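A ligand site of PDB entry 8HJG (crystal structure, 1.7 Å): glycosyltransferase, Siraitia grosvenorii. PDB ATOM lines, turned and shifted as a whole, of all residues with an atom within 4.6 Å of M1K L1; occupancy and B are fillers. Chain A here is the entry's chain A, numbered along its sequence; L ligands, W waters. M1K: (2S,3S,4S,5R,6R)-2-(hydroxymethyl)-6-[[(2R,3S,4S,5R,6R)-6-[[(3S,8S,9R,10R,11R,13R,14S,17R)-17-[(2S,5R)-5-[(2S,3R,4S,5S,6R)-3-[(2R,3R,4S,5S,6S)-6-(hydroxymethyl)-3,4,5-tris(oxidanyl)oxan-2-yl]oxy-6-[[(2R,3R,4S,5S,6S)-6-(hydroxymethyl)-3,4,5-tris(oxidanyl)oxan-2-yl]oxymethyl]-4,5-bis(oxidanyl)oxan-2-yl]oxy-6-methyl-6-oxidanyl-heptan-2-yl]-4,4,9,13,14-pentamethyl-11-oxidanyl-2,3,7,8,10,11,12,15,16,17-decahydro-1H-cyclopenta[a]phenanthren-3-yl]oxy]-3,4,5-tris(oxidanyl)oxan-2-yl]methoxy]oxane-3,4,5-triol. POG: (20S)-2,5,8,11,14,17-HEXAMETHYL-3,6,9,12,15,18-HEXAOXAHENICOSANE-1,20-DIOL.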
ATOM      1  N   TRP A 126      27.818 -15.344   7.714  1.00  0.00           N
ATOM      2  CA  TRP A 126      27.258 -16.683   7.616  1.00  0.00           C
ATOM      3  C   TRP A 126      25.881 -16.781   8.260  1.00  0.00           C
ATOM      4  O   TRP A 126      25.127 -17.716   7.953  1.00  0.00           O
ATOM      5  CB  TRP A 126      28.198 -17.688   8.271  1.00  0.00           C
ATOM      6  CG  TRP A 126      28.715 -17.255   9.612  1.00  0.00           C
ATOM      7  CD1 TRP A 126      29.858 -16.555   9.870  1.00  0.00           C
ATOM      8  CD2 TRP A 126      28.105 -17.499  10.885  1.00  0.00           C
ATOM      9  NE1 TRP A 126      30.001 -16.366  11.227  1.00  0.00           N
ATOM     10  CE2 TRP A 126      28.925 -16.927  11.869  1.00  0.00           C
ATOM     11  CE3 TRP A 126      26.926 -18.147  11.289  1.00  0.00           C
ATOM     12  CZ2 TRP A 126      28.629 -16.985  13.235  1.00  0.00           C
ATOM     13  CZ3 TRP A 126      26.627 -18.210  12.642  1.00  0.00           C
ATOM     14  CH2 TRP A 126      27.479 -17.633  13.593  1.00  0.00           C
ATOM     15  N   ARG A 129      22.885 -16.284   5.983  1.00  0.00           N
ATOM     16  CA  ARG A 129      22.910 -17.378   4.978  1.00  0.00           C
ATOM     17  C   ARG A 129      22.284 -18.634   5.576  1.00  0.00           C
ATOM     18  O   ARG A 129      21.461 -19.266   4.894  1.00  0.00           O
ATOM     19  CB  ARG A 129      24.328 -17.597   4.455  1.00  0.00           C
ATOM     20  CG  ARG A 129      24.918 -16.387   3.752  1.00  0.00           C
ATOM     21  CD  ARG A 129      25.922 -16.770   2.693  1.00  0.00           C
ATOM     22  NE  ARG A 129      27.238 -17.098   3.230  1.00  0.00           N
ATOM     23  CZ  ARG A 129      28.064 -16.209   3.777  1.00  0.00           C
ATOM     24  NH1 ARG A 129      27.715 -14.939   3.866  1.00  0.00           N
ATOM     25  NH2 ARG A 129      29.241 -16.606   4.242  1.00  0.00           N
ATOM     26  N   LEU A 153      31.209   4.223   4.271  1.00  0.00           N
ATOM     27  CA  LEU A 153      30.606   3.934   2.966  1.00  0.00           C
ATOM     28  C   LEU A 153      30.750   5.105   1.995  1.00  0.00           C
ATOM     29  O   LEU A 153      30.840   4.880   0.782  1.00  0.00           O
ATOM     30  CB  LEU A 153      29.135   3.581   3.151  1.00  0.00           C
ATOM     31  CG  LEU A 153      28.368   3.012   1.957  1.00  0.00           C
ATOM     32  CD1 LEU A 153      29.161   1.885   1.282  1.00  0.00           C
ATOM     33  CD2 LEU A 153      27.021   2.497   2.428  1.00  0.00           C
ATOM     34  N   ILE A 156      33.517   5.095  -0.763  1.00  0.00           N
ATOM     35  CA  ILE A 156      33.311   4.053  -1.769  1.00  0.00           C
ATOM     36  C   ILE A 156      32.570   4.619  -2.964  1.00  0.00           C
ATOM     37  O   ILE A 156      32.858   4.281  -4.125  1.00  0.00           O
ATOM     38  CB  ILE A 156      32.577   2.855  -1.141  1.00  0.00           C
ATOM     39  CG1 ILE A 156      33.468   2.210  -0.088  1.00  0.00           C
ATOM     40  CG2 ILE A 156      32.140   1.861  -2.202  1.00  0.00           C
ATOM     41  CD1 ILE A 156      32.743   1.247   0.814  1.00  0.00           C
ATOM     42  N   HIS A 157      31.611   5.514  -2.717  1.00  0.00           N
ATOM     43  CA  HIS A 157      30.788   6.100  -3.768  1.00  0.00           C
ATOM     44  C   HIS A 157      31.278   7.474  -4.221  1.00  0.00           C
ATOM     45  O   HIS A 157      31.050   7.853  -5.379  1.00  0.00           O
ATOM     46  CB  HIS A 157      29.343   6.204  -3.291  1.00  0.00           C
ATOM     47  CG  HIS A 157      28.664   4.877  -3.139  1.00  0.00           C
ATOM     48  ND1 HIS A 157      28.077   4.212  -4.206  1.00  0.00           N
ATOM     49  CD2 HIS A 157      28.478   4.081  -2.061  1.00  0.00           C
ATOM     50  CE1 HIS A 157      27.565   3.068  -3.786  1.00  0.00           C
ATOM     51  NE2 HIS A 157      27.810   2.959  -2.480  1.00  0.00           N
ATOM     52  N   GLU A 194      33.884  -5.659   3.155  1.00  0.00           N
ATOM     53  CA  GLU A 194      32.854  -6.324   2.329  1.00  0.00           C
ATOM     54  C   GLU A 194      32.023  -7.246   3.237  1.00  0.00           C
ATOM     55  O   GLU A 194      30.802  -7.291   3.052  1.00  0.00           O
ATOM     56  CB  GLU A 194      33.494  -7.154   1.214  1.00  0.00           C
ATOM     57  CG  GLU A 194      34.079  -6.313   0.098  1.00  0.00           C
ATOM     58  CD  GLU A 194      34.755  -7.107  -1.009  1.00  0.00           C
ATOM     59  OE1 GLU A 194      35.014  -8.301  -0.804  1.00  0.00           O
ATOM     60  OE2 GLU A 194      35.002  -6.522  -2.072  1.00  0.00           O
ATOM     61  N   ALA A 195      32.680  -7.926   4.170  1.00  0.00           N
ATOM     62  CA  ALA A 195      31.904  -8.786   5.054  1.00  0.00           C
ATOM     63  C   ALA A 195      30.972  -7.982   5.931  1.00  0.00           C
ATOM     64  O   ALA A 195      29.819  -8.364   6.144  1.00  0.00           O
ATOM     65  CB  ALA A 195      32.838  -9.636   5.927  1.00  0.00           C
ATOM     66  N   LEU A 197      29.732  -4.866   5.273  1.00  0.00           N
ATOM     67  CA  LEU A 197      28.645  -4.302   4.480  1.00  0.00           C
ATOM     68  C   LEU A 197      27.665  -5.384   4.059  1.00  0.00           C
ATOM     69  O   LEU A 197      26.456  -5.136   3.973  1.00  0.00           O
ATOM     70  CB  LEU A 197      29.192  -3.561   3.266  1.00  0.00           C
ATOM     71  CG  LEU A 197      29.919  -2.243   3.547  1.00  0.00           C
ATOM     72  CD1 LEU A 197      30.461  -1.645   2.231  1.00  0.00           C
ATOM     73  CD2 LEU A 197      29.014  -1.239   4.269  1.00  0.00           C
ATOM     74  N   TYR A 198      28.150  -6.613   3.812  1.00  0.00           N
ATOM     75  CA  TYR A 198      27.244  -7.688   3.443  1.00  0.00           C
ATOM     76  C   TYR A 198      26.203  -7.924   4.526  1.00  0.00           C
ATOM     77  O   TYR A 198      25.024  -8.131   4.236  1.00  0.00           O
ATOM     78  CB  TYR A 198      28.015  -8.983   3.176  1.00  0.00           C
ATOM     79  CG  TYR A 198      27.076 -10.149   2.891  1.00  0.00           C
ATOM     80  CD1 TYR A 198      26.500 -10.304   1.649  1.00  0.00           C
ATOM     81  CD2 TYR A 198      26.740 -11.066   3.891  1.00  0.00           C
ATOM     82  CE1 TYR A 198      25.622 -11.343   1.391  1.00  0.00           C
ATOM     83  CE2 TYR A 198      25.879 -12.097   3.649  1.00  0.00           C
ATOM     84  CZ  TYR A 198      25.325 -12.237   2.395  1.00  0.00           C
ATOM     85  OH  TYR A 198      24.463 -13.272   2.131  1.00  0.00           O
ATOM     86  N   HIS A 201      23.653  -5.213   4.016  1.00  0.00           N
ATOM     87  CA  HIS A 201      22.983  -5.334   2.717  1.00  0.00           C
ATOM     88  C   HIS A 201      22.091  -6.569   2.649  1.00  0.00           C
ATOM     89  O   HIS A 201      21.027  -6.520   2.018  1.00  0.00           O
ATOM     90  CB  HIS A 201      24.078  -5.338   1.638  1.00  0.00           C
ATOM     91  CG  HIS A 201      23.634  -5.755   0.266  1.00  0.00           C
ATOM     92  ND1 HIS A 201      23.013  -4.892  -0.612  1.00  0.00           N
ATOM     93  CD2 HIS A 201      23.790  -6.924  -0.396  1.00  0.00           C
ATOM     94  CE1 HIS A 201      22.769  -5.526  -1.746  1.00  0.00           C
ATOM     95  NE2 HIS A 201      23.238  -6.762  -1.648  1.00  0.00           N
ATOM     96  N   VAL A 225      20.252   5.977   1.678  1.00  0.00           N
ATOM     97  CA  VAL A 225      20.353   6.204   0.244  1.00  0.00           C
ATOM     98  C   VAL A 225      21.546   5.457  -0.332  1.00  0.00           C
ATOM     99  O   VAL A 225      21.461   4.832  -1.403  1.00  0.00           O
ATOM    100  CB  VAL A 225      20.471   7.708  -0.055  1.00  0.00           C
ATOM    101  CG1 VAL A 225      20.810   7.904  -1.545  1.00  0.00           C
ATOM    102  CG2 VAL A 225      19.191   8.411   0.307  1.00  0.00           C
ATOM    103  N   LEU A 226      22.693   5.518   0.359  1.00  0.00           N
ATOM    104  CA  LEU A 226      23.885   4.816  -0.110  1.00  0.00           C
ATOM    105  C   LEU A 226      23.641   3.302  -0.195  1.00  0.00           C
ATOM    106  O   LEU A 226      23.983   2.670  -1.194  1.00  0.00           O
ATOM    107  CB  LEU A 226      25.061   5.103   0.815  1.00  0.00           C
ATOM    108  CG  LEU A 226      25.593   6.539   0.877  1.00  0.00           C
ATOM    109  CD1 LEU A 226      26.652   6.691   1.973  1.00  0.00           C
ATOM    110  CD2 LEU A 226      26.150   6.943  -0.485  1.00  0.00           C
ATOM    111  N   LEU A 227      23.032   2.716   0.832  1.00  0.00           N
ATOM    112  CA  LEU A 227      22.755   1.285   0.813  1.00  0.00           C
ATOM    113  C   LEU A 227      21.487   0.917   0.046  1.00  0.00           C
ATOM    114  O   LEU A 227      21.286  -0.271  -0.221  1.00  0.00           O
ATOM    115  CB  LEU A 227      22.609   0.725   2.236  1.00  0.00           C
ATOM    116  CG  LEU A 227      23.925   0.577   2.979  1.00  0.00           C
ATOM    117  CD1 LEU A 227      23.645   0.196   4.426  1.00  0.00           C
ATOM    118  CD2 LEU A 227      24.790  -0.465   2.291  1.00  0.00           C
ATOM    119  N   ASN A 228      20.641   1.878  -0.289  1.00  0.00           N
ATOM    120  CA  ASN A 228      19.326   1.585  -0.857  1.00  0.00           C
ATOM    121  C   ASN A 228      18.568   0.591   0.019  1.00  0.00           C
ATOM    122  O   ASN A 228      17.979  -0.389  -0.472  1.00  0.00           O
ATOM    123  CB  ASN A 228      19.442   1.074  -2.306  1.00  0.00           C
ATOM    124  CG  ASN A 228      18.113   1.081  -3.024  1.00  0.00           C
ATOM    125  OD1 ASN A 228      17.277   1.957  -2.806  1.00  0.00           O
ATOM    126  ND2 ASN A 228      17.893   0.087  -3.883  1.00  0.00           N
HETATM  127  C30 M1K L   1      27.950  -4.641  -1.124  1.00  0.00           C
HETATM  128  C31 M1K L   1      29.207  -5.274  -1.495  1.00  0.00           C
HETATM  129  C32 M1K L   1      28.049  -3.127  -1.053  1.00  0.00           C
HETATM  130  C33 M1K L   1      28.536  -2.464  -2.346  1.00  0.00           C
HETATM  131  C34 M1K L   1      28.749  -6.729  -1.417  1.00  0.00           C
HETATM  132  C35 M1K L   1      29.549  -4.707  -2.879  1.00  0.00           C
HETATM  133  C36 M1K L   1      27.663  -5.269   0.258  1.00  0.00           C
HETATM  134  C37 M1K L   1      29.793  -3.177  -2.801  1.00  0.00           C
HETATM  135  C38 M1K L   1      27.415  -2.270  -3.326  1.00  0.00           C
HETATM  136  C39 M1K L   1      28.039  -6.746   0.017  1.00  0.00           C
HETATM  137  C40 M1K L   1      26.702  -2.522  -0.531  1.00  0.00           C
HETATM  138  C41 M1K L   1      26.792  -5.223  -2.067  1.00  0.00           C
HETATM  139  C42 M1K L   1      30.290  -4.895  -0.432  1.00  0.00           C
HETATM  140  C43 M1K L   1      29.696  -7.951  -1.590  1.00  0.00           C
HETATM  141  C44 M1K L   1      25.985  -2.003  -2.867  1.00  0.00           C
HETATM  142  C45 M1K L   1      28.911  -1.061  -1.928  1.00  0.00           C
HETATM  143  C46 M1K L   1      27.698  -1.084  -4.216  1.00  0.00           C
HETATM  144  C47 M1K L   1      25.676  -2.076  -1.445  1.00  0.00           C
HETATM  145  C48 M1K L   1      24.909  -1.898  -3.795  1.00  0.00           C
HETATM  146  C49 M1K L   1      26.575  -1.148  -5.273  1.00  0.00           C
HETATM  147  C50 M1K L   1      25.234  -0.923  -4.761  1.00  0.00           C
HETATM  148  C51 M1K L   1      29.735  -8.782  -0.264  1.00  0.00           C
HETATM  149  C52 M1K L   1      31.077  -7.695  -2.129  1.00  0.00           C
HETATM  150  C53 M1K L   1      24.627  -3.230  -4.501  1.00  0.00           C
HETATM  151  C54 M1K L   1      23.723  -1.527  -3.028  1.00  0.00           C
HETATM  152  C55 M1K L   1      30.701  -9.937  -0.384  1.00  0.00           C
HETATM  153  C56 M1K L   1      30.068 -11.302   0.120  1.00  0.00           C
HETATM  154  C57 M1K L   1      24.528   1.477  -5.151  1.00  0.00           C
HETATM  155  C58 M1K L   1      31.256 -12.192   0.780  1.00  0.00           C
HETATM  156  C59 M1K L   1      24.047   2.626  -4.383  1.00  0.00           C
HETATM  157  C60 M1K L   1      23.564   3.887  -5.401  1.00  0.00           C
HETATM  158  C61 M1K L   1      31.877 -11.411   1.970  1.00  0.00           C
HETATM  159  C62 M1K L   1      32.332 -12.487  -0.271  1.00  0.00           C
HETATM  160  C63 M1K L   1      24.963   2.899  -7.091  1.00  0.00           C
HETATM  161  C64 M1K L   1      24.645   4.155  -6.382  1.00  0.00           C
HETATM  162  C65 M1K L   1      28.388 -12.840  -0.685  1.00  0.00           C
HETATM  163  C66 M1K L   1      27.330 -12.759  -1.764  1.00  0.00           C
HETATM  164  C67 M1K L   1      25.986   3.175  -8.211  1.00  0.00           C
HETATM  165  C68 M1K L   1      26.252 -13.861  -1.525  1.00  0.00           C
HETATM  166  C69 M1K L   1      28.011 -15.068  -0.157  1.00  0.00           C
HETATM  167  C70 M1K L   1      26.942 -15.233  -1.237  1.00  0.00           C
HETATM  168  C71 M1K L   1      28.767 -16.437   0.083  1.00  0.00           C
HETATM  169  C72 M1K L   1      26.281 -11.031  -2.951  1.00  0.00           C
HETATM  170  C73 M1K L   1      27.972   4.426  -8.326  1.00  0.00           C
HETATM  171  C74 M1K L   1      24.997 -10.164  -2.675  1.00  0.00           C
HETATM  172  C75 M1K L   1      29.085   4.961  -7.534  1.00  0.00           C
HETATM  173  C76 M1K L   1      24.600  -9.478  -3.967  1.00  0.00           C
HETATM  174  C77 M1K L   1      30.035   5.793  -8.414  1.00  0.00           C
HETATM  175  C78 M1K L   1      27.109  -8.927  -4.014  1.00  0.00           C
HETATM  176  C79 M1K L   1      29.983   3.657  -9.681  1.00  0.00           C
HETATM  177  C80 M1K L   1      25.703  -8.461  -4.348  1.00  0.00           C
HETATM  178  C81 M1K L   1      30.758   4.815  -9.397  1.00  0.00           C
HETATM  179  C82 M1K L   1      30.871 -17.207   1.169  1.00  0.00           C
HETATM  180  C83 M1K L   1      32.119 -16.720   1.983  1.00  0.00           C
HETATM  181  C84 M1K L   1      28.073  -8.577  -5.130  1.00  0.00           C
HETATM  182  C85 M1K L   1      30.270   3.124 -11.168  1.00  0.00           C
HETATM  183  C86 M1K L   1      33.130 -17.792   2.203  1.00  0.00           C
HETATM  184  C87 M1K L   1      31.002 -18.792   2.973  1.00  0.00           C
HETATM  185  C88 M1K L   1      32.419 -19.111   2.689  1.00  0.00           C
HETATM  186  C89 M1K L   1      30.270 -20.048   3.523  1.00  0.00           C
HETATM  187  O01 M1K L   1      30.270  -2.723  -4.095  1.00  0.00           O
HETATM  188  O02 M1K L   1      25.193   0.532  -4.146  1.00  0.00           O
HETATM  189  O03 M1K L   1      29.473 -11.952  -1.030  1.00  0.00           O
HETATM  190  O04 M1K L   1      25.531   1.883  -6.095  1.00  0.00           O
HETATM  191  O05 M1K L   1      30.731 -13.433   1.301  1.00  0.00           O
HETATM  192  O06 M1K L   1      22.865   2.192  -3.576  1.00  0.00           O
HETATM  193  O07 M1K L   1      23.303   5.029  -4.538  1.00  0.00           O
HETATM  194  O08 M1K L   1      28.920 -14.129  -0.618  1.00  0.00           O
HETATM  195  O09 M1K L   1      24.203   5.111  -7.340  1.00  0.00           O
HETATM  196  O10 M1K L   1      26.784 -11.477  -1.699  1.00  0.00           O
HETATM  197  O11 M1K L   1      27.328   3.425  -7.583  1.00  0.00           O
HETATM  198  O12 M1K L   1      25.375 -14.000  -2.667  1.00  0.00           O
HETATM  199  O13 M1K L   1      25.983 -16.174  -0.780  1.00  0.00           O
HETATM  200  O14 M1K L   1      29.928 -16.133   1.051  1.00  0.00           O
HETATM  201  O15 M1K L   1      27.291 -10.296  -3.724  1.00  0.00           O
HETATM  202  O16 M1K L   1      28.427   3.879  -9.584  1.00  0.00           O
HETATM  203  O17 M1K L   1      23.974 -11.045  -2.260  1.00  0.00           O
HETATM  204  O18 M1K L   1      28.497   5.822  -6.515  1.00  0.00           O
HETATM  205  O19 M1K L   1      23.419  -8.772  -3.770  1.00  0.00           O
HETATM  206  O20 M1K L   1      31.043   6.373  -7.593  1.00  0.00           O
HETATM  207  O21 M1K L   1      30.273 -18.292   1.828  1.00  0.00           O
HETATM  208  O22 M1K L   1      25.545  -8.129  -5.745  1.00  0.00           O
HETATM  209  O23 M1K L   1      31.119   5.589 -10.575  1.00  0.00           O
HETATM  210  O24 M1K L   1      32.804 -15.696   1.214  1.00  0.00           O
HETATM  211  O25 M1K L   1      28.977  -9.755  -5.462  1.00  0.00           O
HETATM  212  O26 M1K L   1      28.997   3.051 -11.903  1.00  0.00           O
HETATM  213  O27 M1K L   1      34.086 -17.378   3.170  1.00  0.00           O
HETATM  214  O28 M1K L   1      32.502 -20.159   1.668  1.00  0.00           O
HETATM  215  O29 M1K L   1      29.396 -19.570   4.543  1.00  0.00           O
HETATM  216  OH  POG L   2      30.630  -5.717  -6.965  1.00  0.00           O
HETATM  217  C2  POG L   2      30.327  -4.335  -6.794  1.00  0.00           C
HETATM  218  C1  POG L   2      28.846  -4.133  -6.736  1.00  0.00           C
HETATM  219  C3  POG L   2      30.969  -3.514  -7.891  1.00  0.00           C
HETATM  220  O2  POG L   2      30.149  -2.384  -8.155  1.00  0.00           O
HETATM  221  C5  POG L   2      30.777  -1.394  -8.968  1.00  0.00           C
HETATM  222  O1  POG L   2      31.421   0.772   5.895  1.00  0.00           O
HETATM  223  C4  POG L   2      32.416   0.371   4.955  1.00  0.00           C
HETATM  224  C6  POG L   2      33.781   0.321   5.597  1.00  0.00           C
HETATM  225  O3  POG L   2      34.770   0.113   4.568  1.00  0.00           O
HETATM  226  C7  POG L   2      34.389  -0.860   3.611  1.00  0.00           C
HETATM  227  C8  POG L   2      35.395  -0.894   2.471  1.00  0.00           C
HETATM  228  O4  POG L   2      34.944  -1.861   1.519  1.00  0.00           O
HETATM  229  C9  POG L   2      35.387  -1.602   0.199  1.00  0.00           C
HETATM  230  C10 POG L   2      34.607  -2.485  -0.770  1.00  0.00           C
HETATM  231  O5  POG L   2      34.741  -1.968  -2.101  1.00  0.00           O
HETATM  232  C11 POG L   2      33.509  -1.978  -2.811  1.00  0.00           C
HETATM  233  C12 POG L   2      33.714  -1.508  -4.232  1.00  0.00           C
HETATM  234  O6  POG L   2      32.511  -0.864  -4.672  1.00  0.00           O
HETATM  235  C13 POG L   2      32.730   0.130  -5.670  1.00  0.00           C
HETATM  236  C14 POG L   2      31.391   0.763  -6.019  1.00  0.00           C
HETATM  237  O7  POG L   2      30.725  -0.029  -7.021  1.00  0.00           O
HETATM  238  C15 POG L   2      31.576  -0.472  -8.060  1.00  0.00           C
HETATM  239  C16 POG L   2      29.709  -0.637  -9.707  1.00  0.00           C
HETATM  240  C17 POG L   2      31.545   2.179  -6.469  1.00  0.00           C
HETATM  241  C18 POG L   2      33.985  -2.660  -5.148  1.00  0.00           C
HETATM  242  C19 POG L   2      33.144  -2.508  -0.415  1.00  0.00           C
HETATM  243  C20 POG L   2      36.759  -1.281   2.952  1.00  0.00           C
HETATM  244  C21 POG L   2      33.877  -0.740   6.656  1.00  0.00           C
HETATM  245  O   HOH W   1      23.670  -9.421  -7.746  1.00  0.00           O
HETATM  246  O   HOH W   2      26.479 -18.462  -2.153  1.00  0.00           O
HETATM  247  O   HOH W   3      26.720  -5.963  -6.655  1.00  0.00           O
HETATM  248  O   HOH W   4      28.782 -20.995   6.926  1.00  0.00           O
HETATM  249  O   HOH W   5      30.267 -11.503  -3.574  1.00  0.00           O
HETATM  250  O   HOH W   6      33.548   4.837  -6.731  1.00  0.00           O
HETATM  251  O   HOH W   7      22.608  -6.239  -5.500  1.00  0.00           O
HETATM  252  O   HOH W   8      27.026 -20.161   2.949  1.00  0.00           O
HETATM  253  O   HOH W   9      26.201   1.121  -1.371  1.00  0.00           O
HETATM  254  O   HOH W  10      23.039 -12.995  -0.271  1.00  0.00           O
HETATM  255  O   HOH W  11      26.933   1.430 -11.021  1.00  0.00           O
HETATM  256  O   HOH W  12      20.894   0.509  -5.095  1.00  0.00           O
HETATM  257  O   HOH W  13      20.499   4.971  -3.960  1.00  0.00           O
HETATM  258  O   HOH W  14      23.445 -18.174   0.388  1.00  0.00           O
HETATM  259  O   HOH W  15      23.373 -15.802  -0.628  1.00  0.00           O
HETATM  260  O   HOH W  16      22.126 -10.093  -0.415  1.00  0.00           O
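Water W13 bridges the backbone carbonyl oxygen (O) of Val 225 and an oxygen (O07) of M1K L1. Water W8 bridges an oxygen (O29) of M1K L1 (2.9 Å) and the guanidinium group of Arg 129 (3.1 Å). Water W10 lies within hydrogen-bond range of the side-chain hydroxyl of Tyr 198 (2.8 Å) and an oxygen (O17) of M1K L1 (2.9 Å). Water W12 lies within hydrogen-bond range of an oxygen (O06) of M1K L1 and the side-chain amide nitrogen of Asn 228. Water W9 lies within hydrogen-bond range of a ring nitrogen (NE2) of His 157, the backbone carbonyl oxygen (O) of Leu 226 and an oxygen (O02) of M1K L1. Water W6 bridges the backbone carbonyl oxygen (O) of Ile 156 (2.8 Å) and an oxygen (O20) of M1K L1 (3.1 Å).
Glu 194 touches M1K L1 (O to C51, 3.8 Å). CB of Leu 197 touches C36 of M1K L1, 3.8 Å away. CE1 of Tyr 198 touches O10 of M1K L1, 3.3 Å away. Val 225 touches M1K L1 (O to O07, 3.6 Å). O of Leu 227 touches C54 of M1K L1, 3.9 Å away. Asn 228 touches M1K L1 (CB to O06, 3.8 Å). Hydrophobic or aromatic side chains that line M1K L1: His 157, Leu 197, Tyr 198, His 201 and Leu 227. Of the 14 residues printed, 10 come within 4 Å of M1K L1. The nearest printed residue that does not touch M1K L1 is Ala 195 (4.05 Å).
An oxygen (O01) of M1K L1 sits at hydrogen-bond distance from an oxygen (O6) of POG L2 (3.0 Å).
The backbone carbonyl oxygen of His 157 lies within hydrogen-bond range of an oxygen (O20) of M1K L1, at 2.7 Å. An oxygen (O18) of M1K L1 lies within hydrogen-bond range of a ring nitrogen (ND1) of His 157 (2.8 Å). The backbone carbonyl oxygen of Leu 226 is in hydrogen-bond range of an oxygen (O06) of M1K L1, 2.7 Å away. NE2 of His 201 lies within hydrogen-bond range of O19 of M1K L1. O29 of M1K L1 sits at hydrogen-bond distance from NH2 of Arg 129, at 3.0 Å.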
